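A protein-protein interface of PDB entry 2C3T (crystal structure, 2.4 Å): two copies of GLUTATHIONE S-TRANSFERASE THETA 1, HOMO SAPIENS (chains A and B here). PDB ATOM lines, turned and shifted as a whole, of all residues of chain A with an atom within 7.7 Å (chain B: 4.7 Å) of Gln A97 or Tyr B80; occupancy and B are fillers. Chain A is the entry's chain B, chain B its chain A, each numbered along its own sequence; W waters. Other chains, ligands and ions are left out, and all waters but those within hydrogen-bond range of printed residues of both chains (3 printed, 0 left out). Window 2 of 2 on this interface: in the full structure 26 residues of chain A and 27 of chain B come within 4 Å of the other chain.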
ATOM      1  N   PRO A  93     -26.288 -29.934  29.116  1.00  0.00           N
ATOM      2  CA  PRO A  93     -26.788 -30.409  27.748  1.00  0.00           C
ATOM      3  C   PRO A  93     -25.746 -31.065  26.844  1.00  0.00           C
ATOM      4  O   PRO A  93     -24.575 -30.828  26.997  1.00  0.00           O
ATOM      5  CB  PRO A  93     -27.328 -29.110  27.109  1.00  0.00           C
ATOM      6  CG  PRO A  93     -27.720 -28.259  28.305  1.00  0.00           C
ATOM      7  CD  PRO A  93     -26.668 -28.526  29.368  1.00  0.00           C
ATOM      8  N   GLN A  94     -26.228 -31.941  25.941  1.00  0.00           N
ATOM      9  CA  GLN A  94     -25.378 -32.658  24.982  1.00  0.00           C
ATOM     10  C   GLN A  94     -24.877 -31.703  23.936  1.00  0.00           C
ATOM     11  O   GLN A  94     -23.751 -31.809  23.483  1.00  0.00           O
ATOM     12  CB  GLN A  94     -26.135 -33.804  24.323  1.00  0.00           C
ATOM     13  CG  GLN A  94     -26.694 -34.865  25.295  1.00  0.00           C
ATOM     14  CD  GLN A  94     -27.388 -36.014  24.554  1.00  0.00           C
ATOM     15  OE1 GLN A  94     -27.120 -36.250  23.381  1.00  0.00           O
ATOM     16  NE2 GLN A  94     -28.217 -36.777  25.268  1.00  0.00           N
ATOM     17  N   ASP A  95     -25.750 -30.782  23.532  1.00  0.00           N
ATOM     18  CA  ASP A  95     -25.449 -29.772  22.567  1.00  0.00           C
ATOM     19  C   ASP A  95     -24.113 -29.087  22.937  1.00  0.00           C
ATOM     20  O   ASP A  95     -23.988 -28.508  24.034  1.00  0.00           O
ATOM     21  CB  ASP A  95     -26.560 -28.771  22.530  1.00  0.00           C
ATOM     22  CG  ASP A  95     -26.356 -27.730  21.514  1.00  0.00           C
ATOM     23  OD1 ASP A  95     -26.110 -28.085  20.342  1.00  0.00           O
ATOM     24  OD2 ASP A  95     -26.645 -26.557  21.816  1.00  0.00           O
ATOM     25  N   LEU A  96     -23.153 -29.083  22.025  1.00  0.00           N
ATOM     26  CA  LEU A  96     -21.804 -28.476  22.343  1.00  0.00           C
ATOM     27  C   LEU A  96     -21.846 -26.977  22.790  1.00  0.00           C
ATOM     28  O   LEU A  96     -21.229 -26.623  23.783  1.00  0.00           O
ATOM     29  CB  LEU A  96     -20.789 -28.684  21.162  1.00  0.00           C
ATOM     30  CG  LEU A  96     -20.583 -30.171  20.876  1.00  0.00           C
ATOM     31  CD1 LEU A  96     -19.473 -30.360  19.918  1.00  0.00           C
ATOM     32  CD2 LEU A  96     -20.293 -30.949  22.182  1.00  0.00           C
ATOM     33  N   GLN A  97     -22.585 -26.150  22.070  1.00  0.00           N
ATOM     34  CA  GLN A  97     -22.680 -24.701  22.397  1.00  0.00           C
ATOM     35  C   GLN A  97     -23.482 -24.436  23.689  1.00  0.00           C
ATOM     36  O   GLN A  97     -23.149 -23.514  24.449  1.00  0.00           O
ATOM     37  CB  GLN A  97     -23.263 -23.931  21.211  1.00  0.00           C
ATOM     38  CG  GLN A  97     -22.402 -24.076  19.961  1.00  0.00           C
ATOM     39  CD  GLN A  97     -22.886 -23.263  18.818  1.00  0.00           C
ATOM     40  OE1 GLN A  97     -23.883 -22.535  18.926  1.00  0.00           O
ATOM     41  NE2 GLN A  97     -22.152 -23.316  17.710  1.00  0.00           N
ATOM     42  N   ALA A  98     -24.505 -25.262  23.940  1.00  0.00           N
ATOM     43  CA  ALA A  98     -25.333 -25.152  25.155  1.00  0.00           C
ATOM     44  C   ALA A  98     -24.499 -25.583  26.347  1.00  0.00           C
ATOM     45  O   ALA A  98     -24.621 -25.032  27.455  1.00  0.00           O
ATOM     46  CB  ALA A  98     -26.556 -25.976  25.042  1.00  0.00           C
ATOM     47  N   ARG A  99     -23.654 -26.581  26.117  1.00  0.00           N
ATOM     48  CA  ARG A  99     -22.755 -27.088  27.127  1.00  0.00           C
ATOM     49  C   ARG A  99     -21.613 -26.065  27.369  1.00  0.00           C
ATOM     50  O   ARG A  99     -21.202 -25.851  28.498  1.00  0.00           O
ATOM     51  CB  ARG A  99     -22.219 -28.443  26.716  1.00  0.00           C
ATOM     52  CG  ARG A  99     -21.210 -28.970  27.596  1.00  0.00           C
ATOM     53  CD  ARG A  99     -20.909 -30.377  27.287  1.00  0.00           C
ATOM     54  NE  ARG A  99     -22.042 -31.211  27.592  1.00  0.00           N
ATOM     55  CZ  ARG A  99     -22.035 -32.522  27.526  1.00  0.00           C
ATOM     56  NH1 ARG A  99     -20.933 -33.167  27.151  1.00  0.00           N
ATOM     57  NH2 ARG A  99     -23.127 -33.199  27.846  1.00  0.00           N
ATOM     58  N   ALA A 100     -21.162 -25.405  26.289  1.00  0.00           N
ATOM     59  CA  ALA A 100     -20.104 -24.374  26.365  1.00  0.00           C
ATOM     60  C   ALA A 100     -20.565 -23.203  27.214  1.00  0.00           C
ATOM     61  O   ALA A 100     -19.773 -22.603  27.922  1.00  0.00           O
ATOM     62  CB  ALA A 100     -19.707 -23.905  24.991  1.00  0.00           C
ATOM     63  N   ARG A 101     -21.863 -22.878  27.139  1.00  0.00           N
ATOM     64  CA  ARG A 101     -22.430 -21.766  27.954  1.00  0.00           C
ATOM     65  C   ARG A 101     -22.388 -22.074  29.477  1.00  0.00           C
ATOM     66  O   ARG A 101     -22.212 -21.151  30.286  1.00  0.00           O
ATOM     67  CB  ARG A 101     -23.863 -21.387  27.509  1.00  0.00           C
ATOM     68  CG  ARG A 101     -23.894 -20.675  26.206  1.00  0.00           C
ATOM     69  CD  ARG A 101     -25.253 -20.139  25.873  1.00  0.00           C
ATOM     70  NE  ARG A 101     -26.233 -21.175  25.589  1.00  0.00           N
ATOM     71  CZ  ARG A 101     -26.442 -21.681  24.369  1.00  0.00           C
ATOM     72  NH1 ARG A 101     -25.683 -21.283  23.343  1.00  0.00           N
ATOM     73  NH2 ARG A 101     -27.365 -22.610  24.179  1.00  0.00           N
ATOM     74  N   VAL A 102     -22.567 -23.354  29.857  1.00  0.00           N
ATOM     75  CA  VAL A 102     -22.505 -23.731  31.252  1.00  0.00           C
ATOM     76  C   VAL A 102     -21.048 -23.577  31.708  1.00  0.00           C
ATOM     77  O   VAL A 102     -20.776 -22.938  32.703  1.00  0.00           O
ATOM     78  CB  VAL A 102     -23.018 -25.160  31.515  1.00  0.00           C
ATOM     79  CG1 VAL A 102     -22.846 -25.552  33.032  1.00  0.00           C
ATOM     80  CG2 VAL A 102     -24.436 -25.292  31.099  1.00  0.00           C
ATOM     81  N   ASP A 103     -20.108 -24.093  30.899  1.00  0.00           N
ATOM     82  CA  ASP A 103     -18.670 -23.991  31.216  1.00  0.00           C
ATOM     83  C   ASP A 103     -18.216 -22.548  31.271  1.00  0.00           C
ATOM     84  O   ASP A 103     -17.422 -22.178  32.129  1.00  0.00           O
ATOM     85  CB  ASP A 103     -17.822 -24.737  30.192  1.00  0.00           C
ATOM     86  CG  ASP A 103     -18.086 -26.232  30.178  1.00  0.00           C
ATOM     87  OD1 ASP A 103     -18.559 -26.785  31.208  1.00  0.00           O
ATOM     88  OD2 ASP A 103     -17.726 -26.871  29.166  1.00  0.00           O
ATOM     89  N   GLU A 104     -18.745 -21.720  30.362  1.00  0.00           N
ATOM     90  CA  GLU A 104     -18.384 -20.300  30.306  1.00  0.00           C
ATOM     91  C   GLU A 104     -18.702 -19.621  31.605  1.00  0.00           C
ATOM     92  O   GLU A 104     -17.887 -18.865  32.127  1.00  0.00           O
ATOM     93  CB  GLU A 104     -19.119 -19.588  29.165  1.00  0.00           C
ATOM     94  CG  GLU A 104     -18.643 -18.137  28.936  1.00  0.00           C
ATOM     95  CD  GLU A 104     -19.397 -17.441  27.824  1.00  0.00           C
ATOM     96  OE1 GLU A 104     -20.616 -17.728  27.647  1.00  0.00           O
ATOM     97  OE2 GLU A 104     -18.804 -16.528  27.182  1.00  0.00           O
ATOM     98  N   THR A 166     -28.301 -19.920  30.938  1.00  0.00           N
ATOM     99  CA  THR A 166     -27.775 -20.511  29.697  1.00  0.00           C
ATOM    100  C   THR A 166     -28.843 -20.930  28.684  1.00  0.00           C
ATOM    101  O   THR A 166     -28.524 -21.489  27.636  1.00  0.00           O
ATOM    102  CB  THR A 166     -26.860 -21.764  30.006  1.00  0.00           C
ATOM    103  OG1 THR A 166     -27.642 -22.826  30.554  1.00  0.00           O
ATOM    104  CG2 THR A 166     -25.695 -21.400  30.964  1.00  0.00           C
ATOM    105  N   LEU B  64     -13.333 -16.676  21.241  1.00  0.00           N
ATOM    106  CA  LEU B  64     -13.595 -17.578  20.145  1.00  0.00           C
ATOM    107  C   LEU B  64     -14.883 -17.190  19.438  1.00  0.00           C
ATOM    108  O   LEU B  64     -15.844 -16.733  20.080  1.00  0.00           O
ATOM    109  CB  LEU B  64     -13.636 -19.058  20.658  1.00  0.00           C
ATOM    110  CG  LEU B  64     -14.130 -20.241  19.773  1.00  0.00           C
ATOM    111  CD1 LEU B  64     -13.654 -21.587  20.290  1.00  0.00           C
ATOM    112  CD2 LEU B  64     -15.710 -20.242  19.562  1.00  0.00           C
ATOM    113  N   ASP B  66     -17.381 -18.605  16.144  1.00  0.00           N
ATOM    114  CA  ASP B  66     -17.700 -19.534  15.113  1.00  0.00           C
ATOM    115  C   ASP B  66     -19.145 -19.275  14.702  1.00  0.00           C
ATOM    116  O   ASP B  66     -20.085 -19.849  15.277  1.00  0.00           O
ATOM    117  CB  ASP B  66     -17.488 -20.956  15.612  1.00  0.00           C
ATOM    118  CG  ASP B  66     -17.712 -22.009  14.534  1.00  0.00           C
ATOM    119  OD1 ASP B  66     -18.033 -21.650  13.363  1.00  0.00           O
ATOM    120  OD2 ASP B  66     -17.537 -23.204  14.854  1.00  0.00           O
ATOM    121  N   PHE B  69     -22.015 -17.886  17.194  1.00  0.00           N
ATOM    122  CA  PHE B  69     -21.569 -18.385  18.496  1.00  0.00           C
ATOM    123  C   PHE B  69     -20.235 -17.756  18.957  1.00  0.00           C
ATOM    124  O   PHE B  69     -19.198 -17.899  18.298  1.00  0.00           O
ATOM    125  CB  PHE B  69     -21.458 -19.935  18.479  1.00  0.00           C
ATOM    126  CG  PHE B  69     -20.886 -20.515  19.743  1.00  0.00           C
ATOM    127  CD1 PHE B  69     -21.655 -20.562  20.928  1.00  0.00           C
ATOM    128  CD2 PHE B  69     -19.616 -21.109  19.743  1.00  0.00           C
ATOM    129  CE1 PHE B  69     -21.121 -21.104  22.117  1.00  0.00           C
ATOM    130  CE2 PHE B  69     -19.081 -21.682  20.930  1.00  0.00           C
ATOM    131  CZ  PHE B  69     -19.844 -21.686  22.109  1.00  0.00           C
ATOM    132  N   LEU B  71     -17.699 -17.231  22.362  1.00  0.00           N
ATOM    133  CA  LEU B  71     -17.378 -17.830  23.606  1.00  0.00           C
ATOM    134  C   LEU B  71     -16.136 -17.190  24.221  1.00  0.00           C
ATOM    135  O   LEU B  71     -15.205 -16.780  23.503  1.00  0.00           O
ATOM    136  CB  LEU B  71     -17.156 -19.353  23.409  1.00  0.00           C
ATOM    137  CG  LEU B  71     -16.945 -20.285  24.622  1.00  0.00           C
ATOM    138  CD1 LEU B  71     -18.171 -20.316  25.471  1.00  0.00           C
ATOM    139  CD2 LEU B  71     -16.599 -21.690  24.174  1.00  0.00           C
ATOM    140  N   ALA B  76     -13.615 -22.856  29.021  1.00  0.00           N
ATOM    141  CA  ALA B  76     -14.769 -23.202  28.205  1.00  0.00           C
ATOM    142  C   ALA B  76     -14.341 -23.358  26.743  1.00  0.00           C
ATOM    143  O   ALA B  76     -14.857 -24.198  26.040  1.00  0.00           O
ATOM    144  CB  ALA B  76     -15.837 -22.163  28.340  1.00  0.00           C
ATOM    145  N   ILE B  77     -13.365 -22.548  26.307  1.00  0.00           N
ATOM    146  CA  ILE B  77     -12.872 -22.616  24.910  1.00  0.00           C
ATOM    147  C   ILE B  77     -12.133 -23.918  24.660  1.00  0.00           C
ATOM    148  O   ILE B  77     -12.368 -24.603  23.641  1.00  0.00           O
ATOM    149  CB  ILE B  77     -11.959 -21.413  24.543  1.00  0.00           C
ATOM    150  CG1 ILE B  77     -12.747 -20.100  24.596  1.00  0.00           C
ATOM    151  CG2 ILE B  77     -11.378 -21.594  23.182  1.00  0.00           C
ATOM    152  CD1 ILE B  77     -11.906 -18.823  24.212  1.00  0.00           C
ATOM    153  N   LEU B  78     -11.250 -24.273  25.597  1.00  0.00           N
ATOM    154  CA  LEU B  78     -10.476 -25.495  25.506  1.00  0.00           C
ATOM    155  C   LEU B  78     -11.385 -26.728  25.481  1.00  0.00           C
ATOM    156  O   LEU B  78     -11.198 -27.622  24.659  1.00  0.00           O
ATOM    157  CB  LEU B  78      -9.485 -25.576  26.673  1.00  0.00           C
ATOM    158  CG  LEU B  78      -8.351 -24.536  26.666  1.00  0.00           C
ATOM    159  CD1 LEU B  78      -7.556 -24.555  27.981  1.00  0.00           C
ATOM    160  CD2 LEU B  78      -7.431 -24.737  25.453  1.00  0.00           C
ATOM    161  N   LEU B  79     -12.380 -26.762  26.378  1.00  0.00           N
ATOM    162  CA  LEU B  79     -13.310 -27.887  26.440  1.00  0.00           C
ATOM    163  C   LEU B  79     -14.132 -27.952  25.175  1.00  0.00           C
ATOM    164  O   LEU B  79     -14.381 -29.028  24.656  1.00  0.00           O
ATOM    165  CB  LEU B  79     -14.235 -27.786  27.663  1.00  0.00           C
ATOM    166  CG  LEU B  79     -13.601 -27.904  29.062  1.00  0.00           C
ATOM    167  CD1 LEU B  79     -14.659 -27.732  30.174  1.00  0.00           C
ATOM    168  CD2 LEU B  79     -12.921 -29.206  29.207  1.00  0.00           C
ATOM    169  N   TYR B  80     -14.518 -26.788  24.652  1.00  0.00           N
ATOM    170  CA  TYR B  80     -15.325 -26.725  23.417  1.00  0.00           C
ATOM    171  C   TYR B  80     -14.566 -27.278  22.211  1.00  0.00           C
ATOM    172  O   TYR B  80     -15.120 -28.073  21.434  1.00  0.00           O
ATOM    173  CB  TYR B  80     -15.783 -25.289  23.148  1.00  0.00           C
ATOM    174  CG  TYR B  80     -16.514 -25.109  21.838  1.00  0.00           C
ATOM    175  CD1 TYR B  80     -15.855 -24.606  20.710  1.00  0.00           C
ATOM    176  CD2 TYR B  80     -17.838 -25.490  21.704  1.00  0.00           C
ATOM    177  CE1 TYR B  80     -16.515 -24.436  19.517  1.00  0.00           C
ATOM    178  CE2 TYR B  80     -18.505 -25.337  20.510  1.00  0.00           C
ATOM    179  CZ  TYR B  80     -17.838 -24.803  19.415  1.00  0.00           C
ATOM    180  OH  TYR B  80     -18.501 -24.657  18.208  1.00  0.00           O
ATOM    181  N   LEU B  81     -13.301 -26.864  22.061  1.00  0.00           N
ATOM    182  CA  LEU B  81     -12.447 -27.325  20.942  1.00  0.00           C
ATOM    183  C   LEU B  81     -12.196 -28.826  21.022  1.00  0.00           C
ATOM    184  O   LEU B  81     -12.048 -29.486  20.012  1.00  0.00           O
ATOM    185  CB  LEU B  81     -11.131 -26.548  20.915  1.00  0.00           C
ATOM    186  CG  LEU B  81     -11.246 -25.053  20.639  1.00  0.00           C
ATOM    187  CD1 LEU B  81      -9.896 -24.342  20.770  1.00  0.00           C
ATOM    188  CD2 LEU B  81     -11.885 -24.795  19.242  1.00  0.00           C
ATOM    189  N   THR B  82     -12.210 -29.348  22.252  1.00  0.00           N
ATOM    190  CA  THR B  82     -12.021 -30.765  22.552  1.00  0.00           C
ATOM    191  C   THR B  82     -13.193 -31.644  22.129  1.00  0.00           C
ATOM    192  O   THR B  82     -13.031 -32.848  21.857  1.00  0.00           O
ATOM    193  CB  THR B  82     -11.772 -30.972  24.086  1.00  0.00           C
ATOM    194  OG1 THR B  82     -10.531 -30.359  24.458  1.00  0.00           O
ATOM    195  CG2 THR B  82     -11.697 -32.423  24.441  1.00  0.00           C
ATOM    196  N   ARG B  83     -14.342 -31.023  21.974  1.00  0.00           N
ATOM    197  CA  ARG B  83     -15.559 -31.714  21.596  1.00  0.00           C
ATOM    198  C   ARG B  83     -15.899 -31.498  20.101  1.00  0.00           C
ATOM    199  O   ARG B  83     -16.230 -32.453  19.377  1.00  0.00           O
ATOM    200  CB  ARG B  83     -16.668 -31.231  22.499  1.00  0.00           C
ATOM    201  CG  ARG B  83     -16.397 -31.548  23.986  1.00  0.00           C
ATOM    202  CD  ARG B  83     -17.232 -30.701  24.909  1.00  0.00           C
ATOM    203  NE  ARG B  83     -16.998 -31.010  26.337  1.00  0.00           N
ATOM    204  CZ  ARG B  83     -17.377 -30.214  27.342  1.00  0.00           C
ATOM    205  NH1 ARG B  83     -17.794 -28.970  27.081  1.00  0.00           N
ATOM    206  NH2 ARG B  83     -17.156 -30.567  28.584  1.00  0.00           N
ATOM    207  N   LYS B  84     -15.739 -30.259  19.644  1.00  0.00           N
ATOM    208  CA  LYS B  84     -16.015 -29.876  18.268  1.00  0.00           C
ATOM    209  C   LYS B  84     -15.082 -30.544  17.237  1.00  0.00           C
ATOM    210  O   LYS B  84     -15.524 -30.929  16.142  1.00  0.00           O
ATOM    211  CB  LYS B  84     -15.941 -28.327  18.140  1.00  0.00           C
ATOM    212  CG  LYS B  84     -16.180 -27.657  16.681  1.00  0.00           C
ATOM    213  CD  LYS B  84     -17.650 -27.603  16.138  1.00  0.00           C
ATOM    214  CE  LYS B  84     -18.248 -28.933  15.824  1.00  0.00           C
ATOM    215  NZ  LYS B  84     -19.643 -28.771  15.274  1.00  0.00           N
HETATM  216  O   HOH W   1     -18.362 -27.386  24.678  1.00  0.00           O
HETATM  217  O   HOH W   2     -22.197 -21.483  15.496  1.00  0.00           O
HETATM  218  O   HOH W   3     -17.077 -25.819  26.625  1.00  0.00           O
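NH1 of Arg B83 is in salt-bridge range of OD2 of Asp A103, 3.0 Å away.
The backbone NH (N) of Leu B64 lies within hydrogen-bond range of the backbone carbonyl oxygen (O) of Leu B71 (2.9 Å). O of Pro A93 sits at hydrogen-bond distance from NE of Arg A99 (2.6 Å).
Leu A96 touches Lys B84. Phe B69 touches Gln A97 (CG to CD, 3.5 Å). Gln A97 touches Tyr B80 (NE2 to OH, 3.9 Å). Arg A99 touches Arg B83 (CD to NH1, 3.4 Å). Phe B69 touches Ala A100. Ala A100 touches Leu B71. CB of Ala B76 touches O of Ala A100, 3.98 Å away. Ala B76 touches Asp A103 (CB to CB, 3.7 Å). Glu A104 touches Leu B71 (CB to CD1, 3.9 Å). Ala B76 touches Glu A104 (CB to N, 3.6 Å).
Of chain B, only Phe B69 and Tyr B80 come within 4 Å of Gln A97. Tyr B80 touches just one residue of chain A: Gln A97. Printed residues of chain A within 4 Å of Arg B83: Leu A96 (3.6 Å), Arg A99 (3.4 Å) and Asp A103 (3.0 Å). Printed residues of chain A within 4 Å of Phe B69: Gln A97 (3.5 Å) and Ala A100 (3.6 Å). Of the printed residues of chain B, Asp A103 touches Ala B76, Leu B79 and Arg B83. Of the printed residues of chain A, Leu B79 touches Asp A103 (3.3 Å). Of the printed residues of chain B, Ala A100 touches Phe B69 (3.6 Å), Leu B71 (3.7 Å) and Ala B76 (3.98 Å). Leu B64 touches none of the printed residues of chain A. The nearest printed residue of chain A that does not touch Leu B71 is Arg A101 (4.8 Å).
Printed residues of chain B that touch a printed residue of chain A: Phe B69, Leu B71, Ala B76, Leu B79, Tyr B80, Arg B83 and Lys B84. Hydrophobic or aromatic side chains of chain B that line the printed part of chain A: Phe B69, Leu B71, Ala B76, Leu B79 and Tyr B80. Of the 13 printed residues of chain A, 6 touch a printed residue of chain B. Hydrophobic or aromatic side chains of chain A that line the printed part of chain B: Leu A96 and Ala A100. Among the printed residues, Asp or Glu carboxylates within 4 Å of a Lys or Arg side-chain nitrogen of the other chain: Asp A103 with Arg B83 (3.0 Å).
No position is printed for both chains. Of the 13 pairs that touch across the chains among the printed residues, none has its exchanged pair printed and touching as well.
Water W2 lies within hydrogen-bond range of O of Asp B66 and NE2 of Gln A97. Water W3 lies within hydrogen-bond range of the backbone carbonyl oxygen (O) of Ala B76 (2.8 Å), the side-chain carboxylate (OD2) of Asp A103 (2.8 Å), the guanidinium group (NH1) of Arg B83 (3.3 Å) and the backbone NH (N) of Tyr B80 (3.4 Å). Water W1 lies within hydrogen-bond range of NH1 of Arg B83 (2.9 Å) and O of Leu A96 (3.1 Å).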
